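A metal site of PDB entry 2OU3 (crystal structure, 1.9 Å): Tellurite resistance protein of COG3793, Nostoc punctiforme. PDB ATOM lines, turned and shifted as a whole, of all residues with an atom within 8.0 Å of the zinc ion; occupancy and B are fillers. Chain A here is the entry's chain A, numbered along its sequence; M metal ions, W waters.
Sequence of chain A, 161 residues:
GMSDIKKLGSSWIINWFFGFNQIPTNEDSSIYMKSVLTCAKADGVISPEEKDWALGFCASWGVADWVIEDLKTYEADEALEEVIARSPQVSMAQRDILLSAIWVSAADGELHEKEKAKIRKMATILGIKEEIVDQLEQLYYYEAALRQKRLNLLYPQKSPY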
ATOM      1  N   ALA A  40     -36.240 -29.867 -25.442  1.00  0.00           N
ATOM      2  CA  ALA A  40     -34.803 -30.009 -25.225  1.00  0.00           C
ATOM      3  C   ALA A  40     -34.531 -30.809 -23.944  1.00  0.00           C
ATOM      4  O   ALA A  40     -33.684 -31.700 -23.929  1.00  0.00           O
ATOM      5  CB  ALA A  40     -34.127 -28.666 -25.145  1.00  0.00           C
ATOM      6  N   VAL A  45     -32.303 -33.542 -18.285  1.00  0.00           N
ATOM      7  CA  VAL A  45     -32.111 -32.176 -17.850  1.00  0.00           C
ATOM      8  C   VAL A  45     -31.687 -31.298 -19.033  1.00  0.00           C
ATOM      9  O   VAL A  45     -31.404 -31.748 -20.151  1.00  0.00           O
ATOM     10  CB  VAL A  45     -31.033 -32.087 -16.767  1.00  0.00           C
ATOM     11  N   ILE A  46     -31.662 -30.006 -18.743  1.00  0.00           N
ATOM     12  CA  ILE A  46     -31.200 -29.013 -19.682  1.00  0.00           C
ATOM     13  C   ILE A  46     -30.110 -28.268 -18.905  1.00  0.00           C
ATOM     14  O   ILE A  46     -30.315 -27.880 -17.770  1.00  0.00           O
ATOM     15  CB  ILE A  46     -32.378 -28.118 -20.142  1.00  0.00           C
ATOM     16  CG1 ILE A  46     -31.907 -26.977 -21.040  1.00  0.00           C
ATOM     17  CG2 ILE A  46     -33.177 -27.567 -18.950  1.00  0.00           C
ATOM     18  CD1 ILE A  46     -33.079 -26.259 -21.703  1.00  0.00           C
ATOM     19  N   SER A  47     -28.930 -28.141 -19.498  1.00  0.00           N
ATOM     20  CA  SER A  47     -27.833 -27.435 -18.831  1.00  0.00           C
ATOM     21  C   SER A  47     -28.037 -25.915 -18.830  1.00  0.00           C
ATOM     22  O   SER A  47     -28.793 -25.375 -19.653  1.00  0.00           O
ATOM     23  CB  SER A  47     -26.517 -27.734 -19.512  1.00  0.00           C
ATOM     24  OG  SER A  47     -26.523 -27.215 -20.830  1.00  0.00           O
ATOM     25  N   GLU A  49     -25.962 -23.710 -19.839  1.00  0.00           N
ATOM     26  CA  GLU A  49     -25.555 -23.202 -21.134  1.00  0.00           C
ATOM     27  C   GLU A  49     -26.643 -23.369 -22.189  1.00  0.00           C
ATOM     28  O   GLU A  49     -26.840 -22.461 -23.026  1.00  0.00           O
ATOM     29  CB  GLU A  49     -24.274 -23.895 -21.621  1.00  0.00           C
ATOM     30  CG  GLU A  49     -23.806 -23.295 -22.957  1.00  0.00           C
ATOM     31  CD  GLU A  49     -22.413 -23.757 -23.397  1.00  0.00           C
ATOM     32  OE1 GLU A  49     -21.907 -24.759 -22.853  1.00  0.00           O
ATOM     33  OE2 GLU A  49     -21.824 -23.103 -24.272  1.00  0.00           O
ATOM     34  N   GLU A  50     -27.309 -24.507 -22.194  1.00  0.00           N
ATOM     35  CA  GLU A  50     -28.394 -24.761 -23.128  1.00  0.00           C
ATOM     36  C   GLU A  50     -29.508 -23.777 -22.838  1.00  0.00           C
ATOM     37  O   GLU A  50     -30.051 -23.137 -23.746  1.00  0.00           O
ATOM     38  CB  GLU A  50     -28.917 -26.191 -22.998  1.00  0.00           C
ATOM     39  CG  GLU A  50     -28.043 -27.263 -23.647  1.00  0.00           C
ATOM     40  CD  GLU A  50     -28.455 -28.662 -23.239  1.00  0.00           C
ATOM     41  OE1 GLU A  50     -29.004 -28.827 -22.128  1.00  0.00           O
ATOM     42  OE2 GLU A  50     -28.238 -29.591 -24.017  1.00  0.00           O
ATOM     43  N   ALA A 101     -35.275 -26.885 -30.527  1.00  0.00           N
ATOM     44  CA  ALA A 101     -34.842 -27.802 -29.465  1.00  0.00           C
ATOM     45  C   ALA A 101     -33.513 -28.478 -29.786  1.00  0.00           C
ATOM     46  O   ALA A 101     -32.633 -28.623 -28.922  1.00  0.00           O
ATOM     47  CB  ALA A 101     -35.913 -28.880 -29.214  1.00  0.00           C
ATOM     48  N   ILE A 102     -33.342 -28.859 -31.057  1.00  0.00           N
ATOM     49  CA  ILE A 102     -32.062 -29.415 -31.529  1.00  0.00           C
ATOM     50  C   ILE A 102     -30.941 -28.414 -31.349  1.00  0.00           C
ATOM     51  O   ILE A 102     -29.891 -28.751 -30.822  1.00  0.00           O
ATOM     52  CB  ILE A 102     -32.157 -29.829 -33.014  1.00  0.00           C
ATOM     53  CG1 ILE A 102     -33.090 -31.038 -33.135  1.00  0.00           C
ATOM     54  CG2 ILE A 102     -30.742 -30.150 -33.615  1.00  0.00           C
ATOM     55  CD1 ILE A 102     -33.643 -31.298 -34.568  1.00  0.00           C
ATOM     56  N   TRP A 103     -31.166 -27.167 -31.792  1.00  0.00           N
ATOM     57  CA  TRP A 103     -30.164 -26.094 -31.663  1.00  0.00           C
ATOM     58  C   TRP A 103     -29.850 -25.814 -30.190  1.00  0.00           C
ATOM     59  O   TRP A 103     -28.695 -25.644 -29.839  1.00  0.00           O
ATOM     60  CB  TRP A 103     -30.630 -24.815 -32.327  1.00  0.00           C
ATOM     61  CG  TRP A 103     -30.248 -24.682 -33.733  1.00  0.00           C
ATOM     62  CD1 TRP A 103     -30.999 -24.990 -34.817  1.00  0.00           C
ATOM     63  CD2 TRP A 103     -28.983 -24.222 -34.213  1.00  0.00           C
ATOM     64  NE1 TRP A 103     -30.285 -24.705 -35.982  1.00  0.00           N
ATOM     65  CE2 TRP A 103     -29.041 -24.255 -35.633  1.00  0.00           C
ATOM     66  CE3 TRP A 103     -27.810 -23.806 -33.593  1.00  0.00           C
ATOM     67  CZ2 TRP A 103     -27.978 -23.865 -36.408  1.00  0.00           C
ATOM     68  CZ3 TRP A 103     -26.752 -23.411 -34.376  1.00  0.00           C
ATOM     69  CH2 TRP A 103     -26.831 -23.458 -35.763  1.00  0.00           C
ATOM     70  N   VAL A 104     -30.882 -25.782 -29.348  1.00  0.00           N
ATOM     71  CA  VAL A 104     -30.652 -25.619 -27.914  1.00  0.00           C
ATOM     72  C   VAL A 104     -29.779 -26.749 -27.332  1.00  0.00           C
ATOM     73  O   VAL A 104     -28.884 -26.479 -26.556  1.00  0.00           O
ATOM     74  CB  VAL A 104     -31.978 -25.547 -27.146  1.00  0.00           C
ATOM     75  CG1 VAL A 104     -31.731 -25.647 -25.636  1.00  0.00           C
ATOM     76  CG2 VAL A 104     -32.722 -24.219 -27.483  1.00  0.00           C
ATOM     77  N   SER A 105     -30.089 -27.976 -27.685  1.00  0.00           N
ATOM     78  CA  SER A 105     -29.368 -29.138 -27.207  1.00  0.00           C
ATOM     79  C   SER A 105     -27.909 -29.086 -27.683  1.00  0.00           C
ATOM     80  O   SER A 105     -27.005 -29.547 -27.023  1.00  0.00           O
ATOM     81  CB  SER A 105     -30.071 -30.394 -27.700  1.00  0.00           C
ATOM     82  OG  SER A 105     -31.324 -30.567 -27.072  1.00  0.00           O
ATOM     83  N   ALA A 106     -27.699 -28.564 -28.877  1.00  0.00           N
ATOM     84  CA  ALA A 106     -26.350 -28.462 -29.438  1.00  0.00           C
ATOM     85  C   ALA A 106     -25.516 -27.361 -28.788  1.00  0.00           C
ATOM     86  O   ALA A 106     -24.309 -27.323 -28.981  1.00  0.00           O
ATOM     87  CB  ALA A 106     -26.442 -28.185 -30.961  1.00  0.00           C
ATOM     88  N   ALA A 107     -26.144 -26.452 -28.013  1.00  0.00           N
ATOM     89  CA  ALA A 107     -25.490 -25.220 -27.540  1.00  0.00           C
ATOM     90  C   ALA A 107     -24.338 -25.494 -26.601  1.00  0.00           C
ATOM     91  O   ALA A 107     -23.416 -24.688 -26.509  1.00  0.00           O
ATOM     92  CB  ALA A 107     -26.520 -24.279 -26.835  1.00  0.00           C
ATOM     93  N   ASP A 108     -24.417 -26.607 -25.886  1.00  0.00           N
ATOM     94  CA  ASP A 108     -23.390 -26.962 -24.923  1.00  0.00           C
ATOM     95  C   ASP A 108     -22.507 -28.105 -25.432  1.00  0.00           C
ATOM     96  O   ASP A 108     -21.878 -28.785 -24.634  1.00  0.00           O
ATOM     97  CB  ASP A 108     -24.024 -27.329 -23.565  1.00  0.00           C
ATOM     98  CG  ASP A 108     -24.880 -28.597 -23.611  1.00  0.00           C
ATOM     99  OD1 ASP A 108     -25.432 -29.006 -24.676  1.00  0.00           O
ATOM    100  OD2 ASP A 108     -25.029 -29.197 -22.533  1.00  0.00           O
ATOM    101  N   GLY A 109     -22.473 -28.309 -26.747  1.00  0.00           N
ATOM    102  CA  GLY A 109     -21.651 -29.355 -27.359  1.00  0.00           C
ATOM    103  C   GLY A 109     -22.410 -30.217 -28.348  1.00  0.00           C
ATOM    104  O   GLY A 109     -23.632 -30.280 -28.322  1.00  0.00           O
ATOM    105  N   GLU A 110     -21.671 -30.897 -29.212  1.00  0.00           N
ATOM    106  CA  GLU A 110     -22.276 -31.713 -30.280  1.00  0.00           C
ATOM    107  C   GLU A 110     -23.277 -32.737 -29.734  1.00  0.00           C
ATOM    108  O   GLU A 110     -23.080 -33.275 -28.624  1.00  0.00           O
ATOM    109  CB  GLU A 110     -21.185 -32.406 -31.109  1.00  0.00           C
ATOM    110  N   LEU A 111     -24.339 -33.003 -30.488  1.00  0.00           N
ATOM    111  CA  LEU A 111     -25.414 -33.883 -30.008  1.00  0.00           C
ATOM    112  C   LEU A 111     -24.943 -35.311 -29.746  1.00  0.00           C
ATOM    113  O   LEU A 111     -24.428 -35.973 -30.621  1.00  0.00           O
ATOM    114  CB  LEU A 111     -26.577 -33.924 -31.005  1.00  0.00           C
ATOM    115  CG  LEU A 111     -27.184 -32.571 -31.394  1.00  0.00           C
ATOM    116  CD1 LEU A 111     -28.157 -32.743 -32.531  1.00  0.00           C
ATOM    117  CD2 LEU A 111     -27.823 -31.953 -30.177  1.00  0.00           C
ATOM    118  N   HIS A 112     -25.166 -35.777 -28.524  1.00  0.00           N
ATOM    119  CA  HIS A 112     -24.854 -37.130 -28.122  1.00  0.00           C
ATOM    120  C   HIS A 112     -26.005 -38.057 -28.534  1.00  0.00           C
ATOM    121  O   HIS A 112     -27.066 -37.571 -28.925  1.00  0.00           O
ATOM    122  CB  HIS A 112     -24.635 -37.160 -26.606  1.00  0.00           C
ATOM    123  CG  HIS A 112     -23.899 -35.964 -26.063  1.00  0.00           C
ATOM    124  N   GLU A 115     -29.166 -37.297 -26.568  1.00  0.00           N
ATOM    125  CA  GLU A 115     -29.943 -36.141 -27.026  1.00  0.00           C
ATOM    126  C   GLU A 115     -30.676 -36.498 -28.327  1.00  0.00           C
ATOM    127  O   GLU A 115     -31.805 -36.070 -28.531  1.00  0.00           O
ATOM    128  CB  GLU A 115     -29.048 -34.897 -27.195  1.00  0.00           C
ATOM    129  CG  GLU A 115     -28.684 -34.198 -25.872  1.00  0.00           C
ATOM    130  CD  GLU A 115     -27.645 -33.113 -26.071  1.00  0.00           C
ATOM    131  OE1 GLU A 115     -26.626 -33.386 -26.723  1.00  0.00           O
ATOM    132  OE2 GLU A 115     -27.837 -31.978 -25.565  1.00  0.00           O
ATOM    133  N   LYS A 118     -33.742 -38.507 -27.067  1.00  0.00           N
ATOM    134  CA  LYS A 118     -34.713 -37.524 -26.539  1.00  0.00           C
ATOM    135  C   LYS A 118     -35.526 -36.853 -27.621  1.00  0.00           C
ATOM    136  O   LYS A 118     -36.771 -36.757 -27.540  1.00  0.00           O
ATOM    137  CB  LYS A 118     -33.976 -36.419 -25.780  1.00  0.00           C
ATOM    138  CG  LYS A 118     -33.320 -36.878 -24.466  1.00  0.00           C
ATOM    139  CD  LYS A 118     -32.993 -35.728 -23.469  1.00  0.00           C
ATOM    140  CE  LYS A 118     -32.306 -34.527 -24.101  1.00  0.00           C
ATOM    141  NZ  LYS A 118     -31.832 -33.538 -23.071  1.00  0.00           N
HETATM  142 ZN    ZN M   1     -26.597 -30.474 -25.210  1.00  0.00          ZN
HETATM  143  O   HOH W   1     -25.978 -31.368 -23.198  1.00  0.00           O
HETATM  144  O   HOH W   2     -24.895 -31.325 -26.305  1.00  0.00           O
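The zinc ion is bound by OD1 of Asp 108, OE2 of Glu 115, O of Ser 105, water W2, OE2 of Glu 50 and water W1.
The zinc ion has six donor atoms within binding distance.
Water W2 lies within hydrogen-bond range of the backbone carbonyl oxygen of Gly 109 (2.6 Å) and the side-chain carboxylate of Glu 115 (2.7 Å).
OD2 of Asp 108 lies within hydrogen-bond range of OG of Ser 47 (3.0 Å).
The backbone NH of Ser 47 is in hydrogen-bond range of the side-chain carboxylate of Glu 50.
The backbone carbonyl oxygen of Ala 101 is in hydrogen-bond range of the side-chain hydroxyl of Ser 105, at 3.0 Å.
The backbone NH (N) of His 112 sits at hydrogen-bond distance from the side-chain carboxylate (OE1) of Glu 115 (3.3 Å).
Of the 20 residues printed, 4 come within 4 Å of the zinc ion.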
